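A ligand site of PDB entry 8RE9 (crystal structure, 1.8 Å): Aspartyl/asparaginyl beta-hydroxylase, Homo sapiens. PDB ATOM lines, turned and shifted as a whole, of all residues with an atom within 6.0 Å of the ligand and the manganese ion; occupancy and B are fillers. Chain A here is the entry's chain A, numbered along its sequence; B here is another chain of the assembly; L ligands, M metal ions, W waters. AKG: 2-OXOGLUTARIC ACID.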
ATOM      1  N   LEU A 305      24.399  18.325  37.634  1.00  0.00           N
ATOM      2  CA  LEU A 305      24.239  18.101  36.206  1.00  0.00           C
ATOM      3  C   LEU A 305      25.546  18.137  35.424  1.00  0.00           C
ATOM      4  O   LEU A 305      25.531  17.958  34.201  1.00  0.00           O
ATOM      5  CB  LEU A 305      23.279  19.130  35.605  1.00  0.00           C
ATOM      6  CG  LEU A 305      21.868  19.149  36.212  1.00  0.00           C
ATOM      7  CD1 LEU A 305      21.057  20.280  35.577  1.00  0.00           C
ATOM      8  CD2 LEU A 305      21.195  17.750  35.986  1.00  0.00           C
ATOM      9  N   TRP A 311      30.330  25.972  35.417  1.00  0.00           N
ATOM     10  CA  TRP A 311      29.066  26.460  34.878  1.00  0.00           C
ATOM     11  C   TRP A 311      28.348  27.167  36.008  1.00  0.00           C
ATOM     12  O   TRP A 311      28.131  26.564  37.071  1.00  0.00           O
ATOM     13  CB  TRP A 311      28.253  25.277  34.357  1.00  0.00           C
ATOM     14  CG  TRP A 311      26.847  25.522  33.911  1.00  0.00           C
ATOM     15  CD1 TRP A 311      26.277  26.698  33.509  1.00  0.00           C
ATOM     16  CD2 TRP A 311      25.820  24.522  33.817  1.00  0.00           C
ATOM     17  NE1 TRP A 311      24.951  26.495  33.162  1.00  0.00           N
ATOM     18  CE2 TRP A 311      24.648  25.162  33.350  1.00  0.00           C
ATOM     19  CE3 TRP A 311      25.778  23.159  34.096  1.00  0.00           C
ATOM     20  CZ2 TRP A 311      23.448  24.479  33.145  1.00  0.00           C
ATOM     21  CZ3 TRP A 311      24.574  22.469  33.870  1.00  0.00           C
ATOM     22  CH2 TRP A 311      23.435  23.128  33.419  1.00  0.00           C
ATOM     23  N   GLN A 313      25.235  30.471  36.927  1.00  0.00           N
ATOM     24  CA  GLN A 313      24.040  31.113  36.416  1.00  0.00           C
ATOM     25  C   GLN A 313      23.683  32.290  37.318  1.00  0.00           C
ATOM     26  O   GLN A 313      23.830  32.208  38.550  1.00  0.00           O
ATOM     27  CB  GLN A 313      22.880  30.085  36.311  1.00  0.00           C
ATOM     28  CG  GLN A 313      23.228  29.015  35.259  1.00  0.00           C
ATOM     29  CD  GLN A 313      22.091  28.073  34.922  1.00  0.00           C
ATOM     30  OE1 GLN A 313      21.451  27.524  35.801  1.00  0.00           O
ATOM     31  NE2 GLN A 313      21.850  27.876  33.628  1.00  0.00           N
ATOM     32  N   SER A 354      23.816  32.515  31.811  1.00  0.00           N
ATOM     33  CA  SER A 354      24.430  31.207  32.004  1.00  0.00           C
ATOM     34  C   SER A 354      25.824  31.267  31.382  1.00  0.00           C
ATOM     35  O   SER A 354      25.944  31.418  30.162  1.00  0.00           O
ATOM     36  CB  SER A 354      23.602  30.108  31.337  1.00  0.00           C
ATOM     37  OG  SER A 354      24.132  28.842  31.624  1.00  0.00           O
ATOM     38  N   ILE A 355      26.858  31.185  32.208  1.00  0.00           N
ATOM     39  CA  ILE A 355      28.247  31.195  31.716  1.00  0.00           C
ATOM     40  C   ILE A 355      28.811  29.782  31.830  1.00  0.00           C
ATOM     41  O   ILE A 355      28.598  29.089  32.836  1.00  0.00           O
ATOM     42  CB  ILE A 355      29.128  32.230  32.442  1.00  0.00           C
ATOM     43  CG1 ILE A 355      30.488  32.369  31.714  1.00  0.00           C
ATOM     44  CG2 ILE A 355      29.277  31.914  33.937  1.00  0.00           C
ATOM     45  CD1 ILE A 355      31.318  33.537  32.159  1.00  0.00           C
ATOM     46  N   MET A 356      29.512  29.358  30.794  1.00  0.00           N
ATOM     47  CA  MET A 356      30.098  28.027  30.807  1.00  0.00           C
ATOM     48  C   MET A 356      31.512  28.132  30.244  1.00  0.00           C
ATOM     49  O   MET A 356      31.734  28.850  29.270  1.00  0.00           O
ATOM     50  CB  MET A 356      29.253  27.047  29.992  1.00  0.00           C
ATOM     51  CG  MET A 356      29.685  25.574  30.159  1.00  0.00           C
ATOM     52  SD  MET A 356      28.560  24.488  29.218  1.00  0.00           S
ATOM     53  CE  MET A 356      26.984  24.844  29.957  1.00  0.00           C
ATOM     54  N   VAL A 362      28.057  18.867  30.352  1.00  0.00           N
ATOM     55  CA  VAL A 362      26.801  18.761  31.094  1.00  0.00           C
ATOM     56  C   VAL A 362      26.175  17.415  30.744  1.00  0.00           C
ATOM     57  O   VAL A 362      25.917  17.126  29.572  1.00  0.00           O
ATOM     58  CB  VAL A 362      25.864  19.908  30.736  1.00  0.00           C
ATOM     59  CG1 VAL A 362      24.496  19.791  31.458  1.00  0.00           C
ATOM     60  CG2 VAL A 362      26.580  21.306  31.021  1.00  0.00           C
ATOM     61  N   HIS A 365      20.290  15.356  30.499  1.00  0.00           N
ATOM     62  CA  HIS A 365      19.293  15.480  31.561  1.00  0.00           C
ATOM     63  C   HIS A 365      18.025  16.069  30.953  1.00  0.00           C
ATOM     64  O   HIS A 365      18.017  16.502  29.799  1.00  0.00           O
ATOM     65  CB  HIS A 365      19.797  16.368  32.706  1.00  0.00           C
ATOM     66  CG  HIS A 365      20.022  17.790  32.306  1.00  0.00           C
ATOM     67  ND1 HIS A 365      21.120  18.203  31.579  1.00  0.00           N
ATOM     68  CD2 HIS A 365      19.275  18.902  32.532  1.00  0.00           C
ATOM     69  CE1 HIS A 365      21.035  19.507  31.366  1.00  0.00           C
ATOM     70  NE2 HIS A 365      19.936  19.959  31.947  1.00  0.00           N
ATOM     71  N   THR A 366      16.937  16.070  31.739  1.00  0.00           N
ATOM     72  CA  THR A 366      15.715  16.734  31.323  1.00  0.00           C
ATOM     73  C   THR A 366      15.238  17.635  32.452  1.00  0.00           C
ATOM     74  O   THR A 366      15.499  17.375  33.623  1.00  0.00           O
ATOM     75  CB  THR A 366      14.601  15.732  30.934  1.00  0.00           C
ATOM     76  OG1 THR A 366      13.776  15.468  32.073  1.00  0.00           O
ATOM     77  CG2 THR A 366      15.204  14.419  30.422  1.00  0.00           C
ATOM     78  N   GLY A 367      14.542  18.710  32.072  1.00  0.00           N
ATOM     79  CA  GLY A 367      13.921  19.573  33.042  1.00  0.00           C
ATOM     80  C   GLY A 367      12.698  18.888  33.657  1.00  0.00           C
ATOM     81  O   GLY A 367      12.268  17.818  33.233  1.00  0.00           O
ATOM     82  N   ARG A 372       6.995  24.532  29.859  1.00  0.00           N
ATOM     83  CA  ARG A 372       7.791  25.684  29.424  1.00  0.00           C
ATOM     84  C   ARG A 372       8.579  25.287  28.187  1.00  0.00           C
ATOM     85  O   ARG A 372       8.831  24.115  27.947  1.00  0.00           O
ATOM     86  CB  ARG A 372       8.806  26.160  30.511  1.00  0.00           C
ATOM     87  CG  ARG A 372       9.846  25.096  30.935  1.00  0.00           C
ATOM     88  CD  ARG A 372      11.124  25.713  31.473  1.00  0.00           C
ATOM     89  NE  ARG A 372      12.167  24.755  31.826  1.00  0.00           N
ATOM     90  CZ  ARG A 372      12.527  24.485  33.071  1.00  0.00           C
ATOM     91  NH1 ARG A 372      11.920  25.057  34.094  1.00  0.00           N
ATOM     92  NH2 ARG A 372      13.543  23.652  33.295  1.00  0.00           N
ATOM     93  N   ARG A 374      12.324  26.808  26.377  1.00  0.00           N
ATOM     94  CA  ARG A 374      13.511  27.495  26.872  1.00  0.00           C
ATOM     95  C   ARG A 374      14.191  28.197  25.710  1.00  0.00           C
ATOM     96  O   ARG A 374      14.568  27.544  24.730  1.00  0.00           O
ATOM     97  CB  ARG A 374      14.436  26.479  27.535  1.00  0.00           C
ATOM     98  CG  ARG A 374      15.747  27.056  28.046  1.00  0.00           C
ATOM     99  CD  ARG A 374      16.227  26.220  29.220  1.00  0.00           C
ATOM    100  NE  ARG A 374      15.509  26.498  30.459  1.00  0.00           N
ATOM    101  CZ  ARG A 374      15.945  26.101  31.650  1.00  0.00           C
ATOM    102  NH1 ARG A 374      17.007  25.316  31.765  1.00  0.00           N
ATOM    103  NH2 ARG A 374      15.322  26.532  32.744  1.00  0.00           N
ATOM    104  N   HIS A 376      17.411  30.413  24.284  1.00  0.00           N
ATOM    105  CA  HIS A 376      18.813  30.753  24.534  1.00  0.00           C
ATOM    106  C   HIS A 376      19.164  31.888  23.583  1.00  0.00           C
ATOM    107  O   HIS A 376      19.039  31.735  22.374  1.00  0.00           O
ATOM    108  CB  HIS A 376      19.727  29.563  24.241  1.00  0.00           C
ATOM    109  CG  HIS A 376      19.778  28.520  25.321  1.00  0.00           C
ATOM    110  ND1 HIS A 376      20.665  27.464  25.278  1.00  0.00           N
ATOM    111  CD2 HIS A 376      19.108  28.391  26.492  1.00  0.00           C
ATOM    112  CE1 HIS A 376      20.543  26.727  26.371  1.00  0.00           C
ATOM    113  NE2 HIS A 376      19.599  27.265  27.126  1.00  0.00           N
ATOM    114  N   ILE A 388      25.057  22.161  21.768  1.00  0.00           N
ATOM    115  CA  ILE A 388      23.978  21.657  22.609  1.00  0.00           C
ATOM    116  C   ILE A 388      23.171  20.671  21.779  1.00  0.00           C
ATOM    117  O   ILE A 388      22.781  20.981  20.651  1.00  0.00           O
ATOM    118  CB  ILE A 388      23.074  22.792  23.141  1.00  0.00           C
ATOM    119  CG1 ILE A 388      21.824  22.220  23.830  1.00  0.00           C
ATOM    120  CG2 ILE A 388      22.696  23.785  22.013  1.00  0.00           C
ATOM    121  CD1 ILE A 388      21.070  23.311  24.624  1.00  0.00           C
ATOM    122  N   TRP A 397      25.145  27.863  19.133  1.00  0.00           N
ATOM    123  CA  TRP A 397      24.648  29.215  19.335  1.00  0.00           C
ATOM    124  C   TRP A 397      25.306  30.182  18.371  1.00  0.00           C
ATOM    125  O   TRP A 397      26.354  29.913  17.791  1.00  0.00           O
ATOM    126  CB  TRP A 397      24.927  29.663  20.756  1.00  0.00           C
ATOM    127  CG  TRP A 397      24.277  28.836  21.829  1.00  0.00           C
ATOM    128  CD1 TRP A 397      23.065  29.033  22.377  1.00  0.00           C
ATOM    129  CD2 TRP A 397      24.867  27.728  22.527  1.00  0.00           C
ATOM    130  NE1 TRP A 397      22.822  28.112  23.366  1.00  0.00           N
ATOM    131  CE2 TRP A 397      23.916  27.281  23.471  1.00  0.00           C
ATOM    132  CE3 TRP A 397      26.100  27.041  22.423  1.00  0.00           C
ATOM    133  CZ2 TRP A 397      24.139  26.202  24.310  1.00  0.00           C
ATOM    134  CZ3 TRP A 397      26.329  25.975  23.266  1.00  0.00           C
ATOM    135  CH2 TRP A 397      25.356  25.566  24.202  1.00  0.00           C
ATOM    136  N   PHE A 405      14.392  25.486  22.493  1.00  0.00           N
ATOM    137  CA  PHE A 405      14.168  24.047  22.585  1.00  0.00           C
ATOM    138  C   PHE A 405      13.222  23.756  23.740  1.00  0.00           C
ATOM    139  O   PHE A 405      12.964  24.609  24.592  1.00  0.00           O
ATOM    140  CB  PHE A 405      15.466  23.234  22.771  1.00  0.00           C
ATOM    141  CG  PHE A 405      16.261  23.572  24.025  1.00  0.00           C
ATOM    142  CD1 PHE A 405      16.936  24.772  24.125  1.00  0.00           C
ATOM    143  CD2 PHE A 405      16.344  22.661  25.081  1.00  0.00           C
ATOM    144  CE1 PHE A 405      17.682  25.096  25.254  1.00  0.00           C
ATOM    145  CE2 PHE A 405      17.089  22.962  26.227  1.00  0.00           C
ATOM    146  CZ  PHE A 405      17.758  24.197  26.313  1.00  0.00           C
ATOM    147  N   ASP A 407      13.224  21.831  26.889  1.00  0.00           N
ATOM    148  CA  ASP A 407      14.139  21.165  27.800  1.00  0.00           C
ATOM    149  C   ASP A 407      13.480  20.037  28.583  1.00  0.00           C
ATOM    150  O   ASP A 407      14.172  19.397  29.388  1.00  0.00           O
ATOM    151  CB  ASP A 407      14.813  22.203  28.723  1.00  0.00           C
ATOM    152  CG  ASP A 407      14.059  22.477  30.024  1.00  0.00           C
ATOM    153  OD1 ASP A 407      12.800  22.545  30.037  1.00  0.00           O
ATOM    154  OD2 ASP A 407      14.765  22.700  31.047  1.00  0.00           O
ATOM    155  N   HIS A 411      18.609  16.639  26.964  1.00  0.00           N
ATOM    156  CA  HIS A 411      19.553  17.523  26.276  1.00  0.00           C
ATOM    157  C   HIS A 411      20.897  17.488  26.996  1.00  0.00           C
ATOM    158  O   HIS A 411      20.998  17.052  28.141  1.00  0.00           O
ATOM    159  CB  HIS A 411      18.980  18.964  26.164  1.00  0.00           C
ATOM    160  CG  HIS A 411      18.547  19.558  27.466  1.00  0.00           C
ATOM    161  ND1 HIS A 411      17.370  19.207  28.107  1.00  0.00           N
ATOM    162  CD2 HIS A 411      19.127  20.492  28.252  1.00  0.00           C
ATOM    163  CE1 HIS A 411      17.273  19.879  29.242  1.00  0.00           C
ATOM    164  NE2 HIS A 411      18.316  20.678  29.345  1.00  0.00           N
ATOM    165  N   VAL A 413      25.184  19.273  26.869  1.00  0.00           N
ATOM    166  CA  VAL A 413      25.966  20.436  26.424  1.00  0.00           C
ATOM    167  C   VAL A 413      27.455  20.162  26.597  1.00  0.00           C
ATOM    168  O   VAL A 413      27.885  19.521  27.569  1.00  0.00           O
ATOM    169  CB  VAL A 413      25.544  21.717  27.170  1.00  0.00           C
ATOM    170  CG1 VAL A 413      26.446  22.883  26.804  1.00  0.00           C
ATOM    171  CG2 VAL A 413      24.086  22.069  26.824  1.00  0.00           C
ATOM    172  N   ARG A 421      31.941  31.115  27.388  1.00  0.00           N
ATOM    173  CA  ARG A 421      30.738  31.178  26.552  1.00  0.00           C
ATOM    174  C   ARG A 421      29.564  31.648  27.403  1.00  0.00           C
ATOM    175  O   ARG A 421      29.223  30.990  28.400  1.00  0.00           O
ATOM    176  CB  ARG A 421      30.460  29.806  25.915  1.00  0.00           C
ATOM    177  CG  ARG A 421      29.227  29.788  24.997  1.00  0.00           C
ATOM    178  CD  ARG A 421      28.180  28.721  25.480  1.00  0.00           C
ATOM    179  NE  ARG A 421      27.690  29.020  26.827  1.00  0.00           N
ATOM    180  CZ  ARG A 421      26.759  28.308  27.458  1.00  0.00           C
ATOM    181  NH1 ARG A 421      26.203  27.242  26.895  1.00  0.00           N
ATOM    182  NH2 ARG A 421      26.396  28.662  28.677  1.00  0.00           N
ATOM    183  N   ILE A 423      25.506  32.917  27.556  1.00  0.00           N
ATOM    184  CA  ILE A 423      24.194  32.981  26.922  1.00  0.00           C
ATOM    185  C   ILE A 423      23.219  33.583  27.916  1.00  0.00           C
ATOM    186  O   ILE A 423      23.496  33.695  29.116  1.00  0.00           O
ATOM    187  CB  ILE A 423      23.686  31.581  26.439  1.00  0.00           C
ATOM    188  CG1 ILE A 423      23.466  30.636  27.606  1.00  0.00           C
ATOM    189  CG2 ILE A 423      24.680  30.944  25.424  1.00  0.00           C
ATOM    190  CD1 ILE A 423      22.763  29.323  27.179  1.00  0.00           C
ATOM    191  N   ILE A 425      19.258  32.948  29.146  1.00  0.00           N
ATOM    192  CA  ILE A 425      18.234  31.911  29.107  1.00  0.00           C
ATOM    193  C   ILE A 425      16.901  32.545  29.482  1.00  0.00           C
ATOM    194  O   ILE A 425      16.786  33.161  30.544  1.00  0.00           O
ATOM    195  CB  ILE A 425      18.585  30.750  30.043  1.00  0.00           C
ATOM    196  CG1 ILE A 425      19.961  30.150  29.647  1.00  0.00           C
ATOM    197  CG2 ILE A 425      17.461  29.725  29.992  1.00  0.00           C
ATOM    198  CD1 ILE A 425      20.335  28.840  30.384  1.00  0.00           C
ATOM    199  N   ASP B  18      16.654  23.284  36.680  1.00  0.00           N
ATOM    200  CA  ASP B  18      17.061  22.640  35.440  1.00  0.00           C
ATOM    201  C   ASP B  18      16.755  21.157  35.401  1.00  0.00           C
ATOM    202  O   ASP B  18      16.666  20.583  34.300  1.00  0.00           O
ATOM    203  CB  ASP B  18      18.570  22.796  35.210  1.00  0.00           C
ATOM    204  CG  ASP B  18      18.894  23.746  34.067  1.00  0.00           C
ATOM    205  OD1 ASP B  18      18.418  24.902  34.158  1.00  0.00           O
ATOM    206  OD2 ASP B  18      19.620  23.357  33.111  1.00  0.00           O
HETATM  207  C1  AKG L   1      19.628  24.464  29.701  1.00  0.00           C
HETATM  208  O1  AKG L   1      18.625  23.821  30.188  1.00  0.00           O
HETATM  209  O2  AKG L   1      19.569  25.603  29.212  1.00  0.00           O
HETATM  210  C2  AKG L   1      20.961  23.679  29.753  1.00  0.00           C
HETATM  211  O5  AKG L   1      20.988  22.563  30.270  1.00  0.00           O
HETATM  212  C3  AKG L   1      22.195  24.294  29.130  1.00  0.00           C
HETATM  213  C4  AKG L   1      22.622  25.587  29.802  1.00  0.00           C
HETATM  214  C5  AKG L   1      23.773  26.256  29.072  1.00  0.00           C
HETATM  215  O3  AKG L   1      24.200  25.849  28.007  1.00  0.00           O
HETATM  216  O4  AKG L   1      24.281  27.289  29.704  1.00  0.00           O
HETATM  217 MN    MN M   1      19.054  21.918  31.043  1.00  0.00          MN
HETATM  218  O   HOH W   1      17.191  21.714  32.016  1.00  0.00           O
HETATM  219  O   HOH W   2      20.202  26.015  32.335  1.00  0.00           O
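OG of Ser 354 is in hydrogen-bond range of O4 of the ligand, 2.5 Å away. A ring nitrogen (NE2) of His 376 sits at hydrogen-bond distance from an oxygen (O2) of the ligand, 2.7 Å away. The guanidinium group of Arg 421 is in salt-bridge range of an oxygen (O3) of the ligand. The guanidinium group (NH1) of Arg 374 lies within salt-bridge range of an oxygen (O2) of the ligand, 3.6 Å away.
The backbone carbonyl oxygen (O) of Asp 407 lies close to a ring nitrogen (ND1) of His 411 (3.5 Å). NH2 of Arg 421 is in hydrogen-bond range of O of Ser 354 (3.2 Å). The side-chain hydroxyl (OG) of Ser 354 is in hydrogen-bond range of the indole nitrogen (NE1) of Trp 311, at 2.9 Å. OG of Ser 354 is in hydrogen-bond range of NE2 of Gln 313 (3.2 Å). A ring nitrogen (ND1) of His 376 lies within hydrogen-bond range of the indole nitrogen of Trp 397 (3.0 Å). N of Met 356 lies within hydrogen-bond range of O of Arg 421. The backbone NH (N) of Arg 374 is in hydrogen-bond range of the backbone carbonyl oxygen (O) of Phe 405. O of Val 413 lies within hydrogen-bond range of N of Val 362, at 2.9 Å.
NE1 of Trp 311 touches O4 of the ligand (3.6 Å). CE of Met 356 touches O3 of the ligand (3.5 Å). CZ2 of Trp 397 touches O3 of the ligand, 3.7 Å away. Phe 405 touches the ligand. Val 413 touches the ligand. CD1 of Ile 423 touches O4 of the ligand, at 3.6 Å. CD1 of Ile 425 touches O2 of the ligand, at 3.5 Å.
Within 4 Å of the manganese ion: His 365, His 411 and Asp 18 of chain B. The nearest printed residue that does not touch the manganese ion is Arg 374 (4.03 Å).
The manganese ion is bound by water W1, O1 of the ligand, O5 of the ligand, NE2 of His 411, NE2 of His 365 and OD2 of Asp 18 of chain B. The manganese ion has six donor atoms within binding distance.
Water W1 lies within hydrogen-bond range of the backbone carbonyl oxygen of Asp 18 of chain B (2.6 Å) and the side-chain carboxylate of Asp 407 (2.8 Å). Water W2 lies within hydrogen-bond range of the side-chain carboxylate of Asp 18 of chain B (2.8 Å), the side-chain amide nitrogen of Gln 313 (2.8 Å), an oxygen (O2) of the ligand (3.2 Å) and the guanidinium group of Arg 374 (3.3 Å).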
